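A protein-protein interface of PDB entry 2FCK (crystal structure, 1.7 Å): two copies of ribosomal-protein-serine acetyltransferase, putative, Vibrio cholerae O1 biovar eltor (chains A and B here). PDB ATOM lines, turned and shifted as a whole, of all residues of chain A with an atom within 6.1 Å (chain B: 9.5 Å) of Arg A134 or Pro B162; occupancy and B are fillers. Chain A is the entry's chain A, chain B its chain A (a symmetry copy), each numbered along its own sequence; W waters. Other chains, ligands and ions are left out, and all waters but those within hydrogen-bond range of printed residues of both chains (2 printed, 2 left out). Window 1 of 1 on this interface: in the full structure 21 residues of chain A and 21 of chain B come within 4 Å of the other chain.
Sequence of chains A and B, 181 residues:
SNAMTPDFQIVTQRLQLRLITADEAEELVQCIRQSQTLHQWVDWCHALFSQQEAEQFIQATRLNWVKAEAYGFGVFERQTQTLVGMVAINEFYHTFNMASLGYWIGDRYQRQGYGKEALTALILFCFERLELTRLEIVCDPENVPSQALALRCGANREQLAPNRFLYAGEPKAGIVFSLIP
The backbone carbonyl oxygen of Thr A133 lies close to the side-chain amide oxygen of Asn B163 (2.9 Å).
NH1 of Arg A134 lies within hydrogen-bond range of O of Pro B162.
OE2 of Glu A136 lies within salt-bridge range of NE of Arg B164, at 3.7 Å.
N of Arg B164 lies within hydrogen-bond range of O of Lys B172.
The backbone carbonyl oxygen (O) of Gly B174 is in hydrogen-bond range of the backbone NH (N) of Ala B161.
OE2 of Glu A158 is in hydrogen-bond range of OG of Ser A178.
The guanidinium group (NE) of Arg A134 lies close to the side-chain sulfur (SD) of Met A98 (3.7 Å).
The backbone carbonyl oxygen of Ala A99 is in hydrogen-bond range of the backbone NH of Glu A136 (2.9 Å).
NH2 of Arg A134 lies within salt-bridge range of OE1 of Glu A158 (2.8 Å).
Arg B164 touches Phe A96.
Asn A97 touches Leu B166 (CB to CD1, 3.8 Å).
CG of Pro B171 touches OG1 of Thr A133, at 3.6 Å.
Arg A134 touches Ala B161.
Asn B163 touches Arg A134.
NE of Arg A134 touches CD of Arg B164 (3.5 Å).
OE1 of Gln B159 touches CA of Glu A158, at 3.0 Å.
Glu A158 touches Ala B161 (OE1 to CB, 3.8 Å).
Glu A158 touches Pro B162.
Asn B163 touches Ile A180.
Thr A133 touches just these residues of chain B: Asn B163 and Pro B171.
Arg A134 touches just these residues of chain B: Ala B161 (3.8 Å), Pro B162 (2.8 Å), Asn B163 (3.4 Å) and Arg B164 (3.5 Å).
Of the printed residues of chain A, Ala B161 touches Arg A134 (3.8 Å) and Glu A158 (3.8 Å).
Of the printed residues of chain A, Arg B164 touches Phe A96, Arg A134 and Glu A136.
Printed residues of chain A within 4 Å of Leu B166: Asn A97 (3.8 Å).
Val B176 touches none of the printed residues of chain A.
The nearest printed residue of chain A that does not touch Gln B159 is Val A176 (6.3 Å).
Of the 18 printed residues of chain B, 7 touch a printed residue of chain A.
Printed residues of chain B that touch a printed residue of chain A: Gln B159, Ala B161, Pro B162, Asn B163, Arg B164, Leu B166 and Pro B171.
Along chain A the printed residues that touch a printed residue of chain B span positions 96 to 180.
Among the printed residues, 13 pairs touch across the chains.
Among the printed residues, Asp or Glu carboxylates within 4 Å of a Lys or Arg side-chain nitrogen of the other chain: Glu A136 with Arg B164 (3.7 Å).
Positions printed for both chains: 136, 158 and 176.
Water W1 bridges OE2 of Glu A136 and NE of Arg B164.
Water W2 lies within hydrogen-bond range of OG1 of Thr A133, O of Asn B163 and O of Phe A96.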
ATOM      1  N   PHE A  96     -13.893  -1.607  -5.163  1.00  0.00           N
ATOM      2  CA  PHE A  96     -12.747  -0.817  -5.561  1.00  0.00           C
ATOM      3  C   PHE A  96     -12.614  -0.602  -7.077  1.00  0.00           C
ATOM      4  O   PHE A  96     -11.589  -0.143  -7.493  1.00  0.00           O
ATOM      5  CB  PHE A  96     -11.473  -1.454  -5.070  1.00  0.00           C
ATOM      6  CG  PHE A  96     -11.548  -1.864  -3.639  1.00  0.00           C
ATOM      7  CD1 PHE A  96     -11.598  -3.192  -3.298  1.00  0.00           C
ATOM      8  CD2 PHE A  96     -11.650  -0.914  -2.668  1.00  0.00           C
ATOM      9  CE1 PHE A  96     -11.703  -3.558  -1.955  1.00  0.00           C
ATOM     10  CE2 PHE A  96     -11.738  -1.268  -1.324  1.00  0.00           C
ATOM     11  CZ  PHE A  96     -11.777  -2.594  -0.991  1.00  0.00           C
ATOM     12  N   ASN A  97     -13.645  -0.964  -7.836  1.00  0.00           N
ATOM     13  CA  ASN A  97     -13.679  -0.861  -9.289  1.00  0.00           C
ATOM     14  C   ASN A  97     -12.472  -1.535  -9.924  1.00  0.00           C
ATOM     15  O   ASN A  97     -11.830  -0.966 -10.803  1.00  0.00           O
ATOM     16  CB  ASN A  97     -13.761   0.595  -9.728  1.00  0.00           C
ATOM     17  CG  ASN A  97     -14.199   0.725 -11.183  1.00  0.00           C
ATOM     18  OD1 ASN A  97     -15.001  -0.078 -11.670  1.00  0.00           O
ATOM     19  ND2 ASN A  97     -13.629   1.694 -11.897  1.00  0.00           N
ATOM     20  N   MET A  98     -12.147  -2.726  -9.417  1.00  0.00           N
ATOM     21  CA  MET A  98     -10.872  -3.376  -9.709  1.00  0.00           C
ATOM     22  C   MET A  98     -11.162  -4.825 -10.068  1.00  0.00           C
ATOM     23  O   MET A  98     -12.236  -5.320  -9.738  1.00  0.00           O
ATOM     24  CB  MET A  98     -10.054  -3.319  -8.365  1.00  0.00           C
ATOM     25  CG  MET A  98      -8.790  -3.936  -8.501  1.00  0.00           C
ATOM     26  SD  MET A  98      -7.771  -3.623  -6.859  1.00  0.00           S
ATOM     27  CE  MET A  98      -7.011  -5.202  -7.089  1.00  0.00           C
ATOM     28  N   ALA A  99     -10.223  -5.538 -10.689  1.00  0.00           N
ATOM     29  CA  ALA A  99     -10.387  -6.983 -10.823  1.00  0.00           C
ATOM     30  C   ALA A  99      -9.026  -7.685 -10.781  1.00  0.00           C
ATOM     31  O   ALA A  99      -8.001  -7.042 -10.930  1.00  0.00           O
ATOM     32  CB  ALA A  99     -11.115  -7.342 -12.197  1.00  0.00           C
ATOM     33  N   SER A 100      -9.081  -8.996 -10.614  1.00  0.00           N
ATOM     34  CA  SER A 100      -7.922  -9.916 -10.551  1.00  0.00           C
ATOM     35  C   SER A 100      -7.805 -10.697 -11.834  1.00  0.00           C
ATOM     36  O   SER A 100      -8.772 -11.328 -12.260  1.00  0.00           O
ATOM     37  CB  SER A 100      -8.233 -10.954  -9.418  1.00  0.00           C
ATOM     38  OG  SER A 100      -7.630 -12.231  -9.702  1.00  0.00           O
ATOM     39  N   PHE A 127     -10.670  -2.275 -19.212  1.00  0.00           N
ATOM     40  CA  PHE A 127     -10.559  -0.797 -19.044  1.00  0.00           C
ATOM     41  C   PHE A 127     -11.591  -0.047 -19.927  1.00  0.00           C
ATOM     42  O   PHE A 127     -12.256   0.896 -19.476  1.00  0.00           O
ATOM     43  CB  PHE A 127      -9.131  -0.284 -19.361  1.00  0.00           C
ATOM     44  CG  PHE A 127      -8.085  -0.631 -18.327  1.00  0.00           C
ATOM     45  CD1 PHE A 127      -8.413  -0.779 -16.963  1.00  0.00           C
ATOM     46  CD2 PHE A 127      -6.738  -0.675 -18.688  1.00  0.00           C
ATOM     47  CE1 PHE A 127      -7.424  -1.040 -16.042  1.00  0.00           C
ATOM     48  CE2 PHE A 127      -5.752  -0.929 -17.745  1.00  0.00           C
ATOM     49  CZ  PHE A 127      -6.095  -1.103 -16.424  1.00  0.00           C
ATOM     50  N   LEU A 132     -13.145  -0.524 -15.563  1.00  0.00           N
ATOM     51  CA  LEU A 132     -12.416  -0.786 -14.336  1.00  0.00           C
ATOM     52  C   LEU A 132     -11.252   0.204 -14.312  1.00  0.00           C
ATOM     53  O   LEU A 132     -10.795   0.664 -15.375  1.00  0.00           O
ATOM     54  CB  LEU A 132     -11.954  -2.250 -14.272  1.00  0.00           C
ATOM     55  CG  LEU A 132     -13.074  -3.279 -14.204  1.00  0.00           C
ATOM     56  CD1 LEU A 132     -12.507  -4.697 -14.388  1.00  0.00           C
ATOM     57  CD2 LEU A 132     -13.924  -3.172 -12.934  1.00  0.00           C
ATOM     58  N   THR A 133     -10.798   0.581 -13.125  1.00  0.00           N
ATOM     59  CA  THR A 133      -9.724   1.563 -13.016  1.00  0.00           C
ATOM     60  C   THR A 133      -8.426   0.993 -12.425  1.00  0.00           C
ATOM     61  O   THR A 133      -7.472   1.713 -12.252  1.00  0.00           O
ATOM     62  CB  THR A 133     -10.174   2.879 -12.261  1.00  0.00           C
ATOM     63  OG1 THR A 133     -10.952   2.543 -11.101  1.00  0.00           O
ATOM     64  CG2 THR A 133     -11.016   3.764 -13.203  1.00  0.00           C
ATOM     65  N   ARG A 134      -8.410  -0.306 -12.148  1.00  0.00           N
ATOM     66  CA  ARG A 134      -7.210  -1.001 -11.713  1.00  0.00           C
ATOM     67  C   ARG A 134      -7.369  -2.501 -11.924  1.00  0.00           C
ATOM     68  O   ARG A 134      -8.434  -3.069 -11.640  1.00  0.00           O
ATOM     69  CB  ARG A 134      -6.987  -0.758 -10.202  1.00  0.00           C
ATOM     70  CG  ARG A 134      -5.745  -1.457  -9.627  1.00  0.00           C
ATOM     71  CD  ARG A 134      -5.453  -1.005  -8.138  1.00  0.00           C
ATOM     72  NE  ARG A 134      -4.499  -1.940  -7.494  1.00  0.00           N
ATOM     73  CZ  ARG A 134      -3.174  -1.779  -7.437  1.00  0.00           C
ATOM     74  NH1 ARG A 134      -2.596  -0.688  -7.921  1.00  0.00           N
ATOM     75  NH2 ARG A 134      -2.413  -2.726  -6.913  1.00  0.00           N
ATOM     76  N   LEU A 135      -6.291  -3.157 -12.365  1.00  0.00           N
ATOM     77  CA  LEU A 135      -6.277  -4.627 -12.425  1.00  0.00           C
ATOM     78  C   LEU A 135      -5.044  -5.116 -11.656  1.00  0.00           C
ATOM     79  O   LEU A 135      -4.016  -4.484 -11.738  1.00  0.00           O
ATOM     80  CB  LEU A 135      -6.156  -5.099 -13.878  1.00  0.00           C
ATOM     81  CG  LEU A 135      -7.284  -4.611 -14.826  1.00  0.00           C
ATOM     82  CD1 LEU A 135      -6.953  -4.950 -16.306  1.00  0.00           C
ATOM     83  CD2 LEU A 135      -8.612  -5.204 -14.462  1.00  0.00           C
ATOM     84  N   GLU A 136      -5.189  -6.208 -10.923  1.00  0.00           N
ATOM     85  CA  GLU A 136      -4.043  -6.903 -10.295  1.00  0.00           C
ATOM     86  C   GLU A 136      -3.781  -8.280 -10.962  1.00  0.00           C
ATOM     87  O   GLU A 136      -4.725  -9.060 -11.206  1.00  0.00           O
ATOM     88  CB  GLU A 136      -4.297  -7.058  -8.813  1.00  0.00           C
ATOM     89  CG  GLU A 136      -4.057  -5.684  -8.133  1.00  0.00           C
ATOM     90  CD  GLU A 136      -4.230  -5.709  -6.611  1.00  0.00           C
ATOM     91  OE1 GLU A 136      -4.575  -6.770  -6.033  1.00  0.00           O
ATOM     92  OE2 GLU A 136      -4.088  -4.613  -6.022  1.00  0.00           O
ATOM     93  N   GLU A 158       4.512  -4.531  -7.855  1.00  0.00           N
ATOM     94  CA  GLU A 158       4.402  -3.996  -6.524  1.00  0.00           C
ATOM     95  C   GLU A 158       4.990  -5.048  -5.600  1.00  0.00           C
ATOM     96  O   GLU A 158       6.156  -5.413  -5.694  1.00  0.00           O
ATOM     97  CB  GLU A 158       2.941  -3.637  -6.172  1.00  0.00           C
ATOM     98  CG  GLU A 158       2.413  -2.482  -7.076  1.00  0.00           C
ATOM     99  CD  GLU A 158       0.954  -2.133  -6.905  1.00  0.00           C
ATOM    100  OE1 GLU A 158       0.278  -2.730  -6.042  1.00  0.00           O
ATOM    101  OE2 GLU A 158       0.484  -1.222  -7.634  1.00  0.00           O
ATOM    102  N   VAL A 176       2.512  -9.263  -6.679  1.00  0.00           N
ATOM    103  CA  VAL A 176       1.402  -8.479  -7.203  1.00  0.00           C
ATOM    104  C   VAL A 176       1.912  -7.474  -8.227  1.00  0.00           C
ATOM    105  O   VAL A 176       2.823  -6.694  -7.917  1.00  0.00           O
ATOM    106  CB  VAL A 176       0.739  -7.710  -6.016  1.00  0.00           C
ATOM    107  CG1 VAL A 176      -0.336  -6.756  -6.522  1.00  0.00           C
ATOM    108  CG2 VAL A 176       0.242  -8.733  -4.989  1.00  0.00           C
ATOM    109  N   PHE A 177       1.336  -7.534  -9.434  1.00  0.00           N
ATOM    110  CA  PHE A 177       1.557  -6.506 -10.445  1.00  0.00           C
ATOM    111  C   PHE A 177       0.239  -5.752 -10.634  1.00  0.00           C
ATOM    112  O   PHE A 177      -0.848  -6.370 -10.546  1.00  0.00           O
ATOM    113  CB  PHE A 177       1.929  -7.159 -11.790  1.00  0.00           C
ATOM    114  CG  PHE A 177       3.227  -7.904 -11.767  1.00  0.00           C
ATOM    115  CD1 PHE A 177       4.388  -7.328 -12.263  1.00  0.00           C
ATOM    116  CD2 PHE A 177       3.267  -9.201 -11.238  1.00  0.00           C
ATOM    117  CE1 PHE A 177       5.583  -8.039 -12.244  1.00  0.00           C
ATOM    118  CE2 PHE A 177       4.431  -9.946 -11.217  1.00  0.00           C
ATOM    119  CZ  PHE A 177       5.632  -9.330 -11.707  1.00  0.00           C
ATOM    120  N   SER A 178       0.322  -4.471 -11.010  1.00  0.00           N
ATOM    121  CA  SER A 178      -0.870  -3.701 -11.298  1.00  0.00           C
ATOM    122  C   SER A 178      -0.854  -3.094 -12.694  1.00  0.00           C
ATOM    123  O   SER A 178       0.201  -2.850 -13.278  1.00  0.00           O
ATOM    124  CB  SER A 178      -1.036  -2.558 -10.275  1.00  0.00           C
ATOM    125  OG  SER A 178      -0.058  -1.565 -10.529  1.00  0.00           O
ATOM    126  N   LEU A 179      -2.059  -2.844 -13.193  1.00  0.00           N
ATOM    127  CA  LEU A 179      -2.257  -2.045 -14.394  1.00  0.00           C
ATOM    128  C   LEU A 179      -3.316  -1.003 -14.066  1.00  0.00           C
ATOM    129  O   LEU A 179      -4.332  -1.333 -13.425  1.00  0.00           O
ATOM    130  CB  LEU A 179      -2.808  -2.945 -15.523  1.00  0.00           C
ATOM    131  CG  LEU A 179      -1.886  -4.057 -15.990  1.00  0.00           C
ATOM    132  CD1 LEU A 179      -2.632  -5.368 -16.132  1.00  0.00           C
ATOM    133  CD2 LEU A 179      -1.284  -3.645 -17.268  1.00  0.00           C
ATOM    134  N   ILE A 180      -3.082   0.234 -14.513  1.00  0.00           N
ATOM    135  CA  ILE A 180      -4.098   1.271 -14.459  1.00  0.00           C
ATOM    136  C   ILE A 180      -4.288   1.889 -15.840  1.00  0.00           C
ATOM    137  O   ILE A 180      -3.392   1.798 -16.684  1.00  0.00           O
ATOM    138  CB  ILE A 180      -3.820   2.380 -13.415  1.00  0.00           C
ATOM    139  CG1 ILE A 180      -2.633   3.255 -13.830  1.00  0.00           C
ATOM    140  CG2 ILE A 180      -3.658   1.753 -12.014  1.00  0.00           C
ATOM    141  CD1 ILE A 180      -2.292   4.389 -12.821  1.00  0.00           C
ATOM    142  N   PRO A 181      -5.475   2.455 -16.092  1.00  0.00           N
ATOM    143  CA  PRO A 181      -5.655   2.964 -17.470  1.00  0.00           C
ATOM    144  C   PRO A 181      -4.715   4.120 -17.843  1.00  0.00           C
ATOM    145  O   PRO A 181      -4.382   4.351 -19.028  1.00  0.00           O
ATOM    146  CB  PRO A 181      -7.116   3.413 -17.496  1.00  0.00           C
ATOM    147  CG  PRO A 181      -7.777   2.710 -16.383  1.00  0.00           C
ATOM    148  CD  PRO A 181      -6.709   2.585 -15.302  1.00  0.00           C
ATOM    149  OXT PRO A 181      -4.249   4.849 -16.963  1.00  0.00           O
ATOM    150  N   GLU B 136      -6.693  -7.681   3.657  1.00  0.00           N
ATOM    151  CA  GLU B 136      -6.094  -6.385   3.270  1.00  0.00           C
ATOM    152  C   GLU B 136      -6.890  -5.192   3.864  1.00  0.00           C
ATOM    153  O   GLU B 136      -8.138  -5.166   3.805  1.00  0.00           O
ATOM    154  CB  GLU B 136      -6.020  -6.291   1.764  1.00  0.00           C
ATOM    155  CG  GLU B 136      -4.842  -7.177   1.280  1.00  0.00           C
ATOM    156  CD  GLU B 136      -4.619  -7.134  -0.236  1.00  0.00           C
ATOM    157  OE1 GLU B 136      -5.382  -6.455  -0.967  1.00  0.00           O
ATOM    158  OE2 GLU B 136      -3.705  -7.867  -0.679  1.00  0.00           O
ATOM    159  N   VAL B 138      -6.889  -0.946   3.245  1.00  0.00           N
ATOM    160  CA  VAL B 138      -6.381   0.119   2.367  1.00  0.00           C
ATOM    161  C   VAL B 138      -6.598   1.437   3.098  1.00  0.00           C
ATOM    162  O   VAL B 138      -7.732   1.752   3.434  1.00  0.00           O
ATOM    163  CB  VAL B 138      -7.132   0.201   0.998  1.00  0.00           C
ATOM    164  CG1 VAL B 138      -6.506   1.288   0.094  1.00  0.00           C
ATOM    165  CG2 VAL B 138      -7.050  -1.175   0.351  1.00  0.00           C
ATOM    166  N   PRO B 141      -3.433   7.608   2.107  1.00  0.00           N
ATOM    167  CA  PRO B 141      -2.081   7.994   2.600  1.00  0.00           C
ATOM    168  C   PRO B 141      -2.087   9.212   3.536  1.00  0.00           C
ATOM    169  O   PRO B 141      -1.146   9.401   4.320  1.00  0.00           O
ATOM    170  CB  PRO B 141      -1.317   8.350   1.311  1.00  0.00           C
ATOM    171  CG  PRO B 141      -2.013   7.638   0.238  1.00  0.00           C
ATOM    172  CD  PRO B 141      -3.472   7.598   0.624  1.00  0.00           C
ATOM    173  N   GLU B 158       2.419  -2.877   3.185  1.00  0.00           N
ATOM    174  CA  GLU B 158       2.982  -3.255   1.917  1.00  0.00           C
ATOM    175  C   GLU B 158       3.015  -1.990   1.079  1.00  0.00           C
ATOM    176  O   GLU B 158       3.654  -1.003   1.422  1.00  0.00           O
ATOM    177  CB  GLU B 158       2.178  -4.395   1.253  1.00  0.00           C
ATOM    178  CG  GLU B 158       2.258  -5.705   2.094  1.00  0.00           C
ATOM    179  CD  GLU B 158       1.405  -6.850   1.605  1.00  0.00           C
ATOM    180  OE1 GLU B 158       0.740  -6.715   0.556  1.00  0.00           O
ATOM    181  OE2 GLU B 158       1.423  -7.916   2.271  1.00  0.00           O
ATOM    182  N   GLN B 159       2.266  -1.995   0.005  1.00  0.00           N
ATOM    183  CA  GLN B 159       2.481  -1.054  -1.037  1.00  0.00           C
ATOM    184  C   GLN B 159       1.722   0.264  -0.907  1.00  0.00           C
ATOM    185  O   GLN B 159       0.682   0.336  -0.242  1.00  0.00           O
ATOM    186  CB  GLN B 159       2.115  -1.739  -2.347  1.00  0.00           C
ATOM    187  CG  GLN B 159       2.825  -1.175  -3.503  1.00  0.00           C
ATOM    188  CD  GLN B 159       4.167  -1.806  -3.801  1.00  0.00           C
ATOM    189  OE1 GLN B 159       4.752  -1.524  -4.837  1.00  0.00           O
ATOM    190  NE2 GLN B 159       4.665  -2.644  -2.906  1.00  0.00           N
ATOM    191  N   LEU B 160       2.258   1.306  -1.543  1.00  0.00           N
ATOM    192  CA  LEU B 160       1.465   2.437  -1.902  1.00  0.00           C
ATOM    193  C   LEU B 160       0.993   2.093  -3.332  1.00  0.00           C
ATOM    194  O   LEU B 160       1.820   2.026  -4.259  1.00  0.00           O
ATOM    195  CB  LEU B 160       2.358   3.683  -1.984  1.00  0.00           C
ATOM    196  CG  LEU B 160       1.664   4.976  -2.433  1.00  0.00           C
ATOM    197  CD1 LEU B 160       0.516   5.281  -1.534  1.00  0.00           C
ATOM    198  CD2 LEU B 160       2.699   6.155  -2.363  1.00  0.00           C
ATOM    199  N   ALA B 161      -0.293   1.878  -3.484  1.00  0.00           N
ATOM    200  CA  ALA B 161      -0.855   1.338  -4.731  1.00  0.00           C
ATOM    201  C   ALA B 161      -1.730   2.374  -5.442  1.00  0.00           C
ATOM    202  O   ALA B 161      -2.743   2.811  -4.891  1.00  0.00           O
ATOM    203  CB  ALA B 161      -1.643   0.136  -4.386  1.00  0.00           C
ATOM    204  N   PRO B 162      -1.383   2.728  -6.695  1.00  0.00           N
ATOM    205  CA  PRO B 162      -2.248   3.675  -7.421  1.00  0.00           C
ATOM    206  C   PRO B 162      -3.643   3.104  -7.719  1.00  0.00           C
ATOM    207  O   PRO B 162      -3.817   1.871  -7.849  1.00  0.00           O
ATOM    208  CB  PRO B 162      -1.481   3.955  -8.723  1.00  0.00           C
ATOM    209  CG  PRO B 162      -0.562   2.821  -8.890  1.00  0.00           C
ATOM    210  CD  PRO B 162      -0.188   2.367  -7.476  1.00  0.00           C
ATOM    211  N   ASN B 163      -4.636   4.003  -7.756  1.00  0.00           N
ATOM    212  CA  ASN B 163      -6.034   3.648  -8.026  1.00  0.00           C
ATOM    213  C   ASN B 163      -6.571   2.510  -7.169  1.00  0.00           C
ATOM    214  O   ASN B 163      -7.404   1.692  -7.582  1.00  0.00           O
ATOM    215  CB  ASN B 163      -6.191   3.308  -9.541  1.00  0.00           C
ATOM    216  CG  ASN B 163      -6.038   4.496 -10.468  1.00  0.00           C
ATOM    217  OD1 ASN B 163      -6.376   4.377 -11.689  1.00  0.00           O
ATOM    218  ND2 ASN B 163      -5.491   5.606  -9.987  1.00  0.00           N
ATOM    219  N   ARG B 164      -6.111   2.430  -5.915  1.00  0.00           N
ATOM    220  CA  ARG B 164      -6.467   1.288  -5.103  1.00  0.00           C
ATOM    221  C   ARG B 164      -7.871   1.336  -4.424  1.00  0.00           C
ATOM    222  O   ARG B 164      -8.424   0.317  -4.029  1.00  0.00           O
ATOM    223  CB  ARG B 164      -5.328   1.033  -4.083  1.00  0.00           C
ATOM    224  CG  ARG B 164      -5.514  -0.186  -3.236  1.00  0.00           C
ATOM    225  CD  ARG B 164      -5.353  -1.448  -4.106  1.00  0.00           C
ATOM    226  NE  ARG B 164      -5.608  -2.605  -3.284  1.00  0.00           N
ATOM    227  CZ  ARG B 164      -6.785  -2.969  -2.815  1.00  0.00           C
ATOM    228  NH1 ARG B 164      -7.874  -2.249  -3.090  1.00  0.00           N
ATOM    229  NH2 ARG B 164      -6.890  -4.043  -2.069  1.00  0.00           N
ATOM    230  N   PHE B 165      -8.456   2.529  -4.253  1.00  0.00           N
ATOM    231  CA  PHE B 165      -9.808   2.565  -3.665  1.00  0.00           C
ATOM    232  C   PHE B 165     -10.609   3.714  -4.271  1.00  0.00           C
ATOM    233  O   PHE B 165     -10.042   4.573  -4.910  1.00  0.00           O
ATOM    234  CB  PHE B 165      -9.784   2.641  -2.104  1.00  0.00           C
ATOM    235  CG  PHE B 165      -9.282   3.977  -1.552  1.00  0.00           C
ATOM    236  CD1 PHE B 165      -7.909   4.269  -1.485  1.00  0.00           C
ATOM    237  CD2 PHE B 165     -10.196   4.949  -1.099  1.00  0.00           C
ATOM    238  CE1 PHE B 165      -7.438   5.502  -0.962  1.00  0.00           C
ATOM    239  CE2 PHE B 165      -9.732   6.186  -0.593  1.00  0.00           C
ATOM    240  CZ  PHE B 165      -8.356   6.459  -0.534  1.00  0.00           C
ATOM    241  N   LEU B 166     -11.931   3.698  -4.073  1.00  0.00           N
ATOM    242  CA  LEU B 166     -12.768   4.797  -4.568  1.00  0.00           C
ATOM    243  C   LEU B 166     -13.160   5.766  -3.439  1.00  0.00           C
ATOM    244  O   LEU B 166     -13.558   5.320  -2.364  1.00  0.00           O
ATOM    245  CB  LEU B 166     -14.037   4.243  -5.219  1.00  0.00           C
ATOM    246  CG  LEU B 166     -13.823   3.236  -6.359  1.00  0.00           C
ATOM    247  CD1 LEU B 166     -15.138   2.523  -6.714  1.00  0.00           C
ATOM    248  CD2 LEU B 166     -13.211   3.980  -7.557  1.00  0.00           C
ATOM    249  N   PRO B 171     -11.015   7.197  -8.364  1.00  0.00           N
ATOM    250  CA  PRO B 171      -9.942   6.379  -7.731  1.00  0.00           C
ATOM    251  C   PRO B 171      -8.751   7.170  -7.164  1.00  0.00           C
ATOM    252  O   PRO B 171      -8.427   8.247  -7.661  1.00  0.00           O
ATOM    253  CB  PRO B 171      -9.514   5.413  -8.862  1.00  0.00           C
ATOM    254  CG  PRO B 171     -10.220   5.976 -10.198  1.00  0.00           C
ATOM    255  CD  PRO B 171     -10.819   7.317  -9.829  1.00  0.00           C
ATOM    256  N   LYS B 172      -8.138   6.647  -6.085  1.00  0.00           N
ATOM    257  CA  LYS B 172      -7.049   7.313  -5.369  1.00  0.00           C
ATOM    258  C   LYS B 172      -6.001   6.289  -4.962  1.00  0.00           C
ATOM    259  O   LYS B 172      -6.367   5.125  -4.782  1.00  0.00           O
ATOM    260  CB  LYS B 172      -7.598   7.940  -4.074  1.00  0.00           C
ATOM    261  CG  LYS B 172      -8.573   9.106  -4.350  1.00  0.00           C
ATOM    262  CD  LYS B 172      -9.503   9.093  -3.185  1.00  0.00           C
ATOM    263  CE  LYS B 172      -8.954   9.955  -2.184  1.00  0.00           C
ATOM    264  NZ  LYS B 172      -9.790  11.301  -1.894  1.00  0.00           N
ATOM    265  N   ALA B 173      -4.739   6.713  -4.860  1.00  0.00           N
ATOM    266  CA  ALA B 173      -3.631   5.859  -4.382  1.00  0.00           C
ATOM    267  C   ALA B 173      -3.859   5.548  -2.906  1.00  0.00           C
ATOM    268  O   ALA B 173      -4.190   6.456  -2.110  1.00  0.00           O
ATOM    269  CB  ALA B 173      -2.335   6.531  -4.577  1.00  0.00           C
ATOM    270  N   GLY B 174      -3.811   4.261  -2.549  1.00  0.00           N
ATOM    271  CA  GLY B 174      -3.978   3.838  -1.131  1.00  0.00           C
ATOM    272  C   GLY B 174      -2.850   2.954  -0.654  1.00  0.00           C
ATOM    273  O   GLY B 174      -2.178   2.279  -1.432  1.00  0.00           O
ATOM    274  N   ILE B 175      -2.593   3.020   0.658  1.00  0.00           N
ATOM    275  CA  ILE B 175      -1.592   2.160   1.247  1.00  0.00           C
ATOM    276  C   ILE B 175      -2.253   0.846   1.646  1.00  0.00           C
ATOM    277  O   ILE B 175      -3.257   0.815   2.368  1.00  0.00           O
ATOM    278  CB  ILE B 175      -1.021   2.772   2.551  1.00  0.00           C
ATOM    279  CG1 ILE B 175      -0.512   4.199   2.318  1.00  0.00           C
ATOM    280  CG2 ILE B 175       0.006   1.785   3.112  1.00  0.00           C
ATOM    281  CD1 ILE B 175      -0.237   5.013   3.643  1.00  0.00           C
ATOM    282  N   VAL B 176      -1.678  -0.245   1.168  1.00  0.00           N
ATOM    283  CA  VAL B 176      -2.171  -1.581   1.471  1.00  0.00           C
ATOM    284  C   VAL B 176      -1.425  -2.153   2.669  1.00  0.00           C
ATOM    285  O   VAL B 176      -0.187  -2.193   2.655  1.00  0.00           O
ATOM    286  CB  VAL B 176      -1.920  -2.493   0.227  1.00  0.00           C
ATOM    287  CG1 VAL B 176      -2.280  -3.940   0.535  1.00  0.00           C
ATOM    288  CG2 VAL B 176      -2.667  -1.898  -0.972  1.00  0.00           C
HETATM  289  O   HOH W   1      -3.561  -4.458  -3.366  1.00  0.00           O
HETATM  290  O   HOH W   2      -9.689   1.214  -9.090  1.00  0.00           O
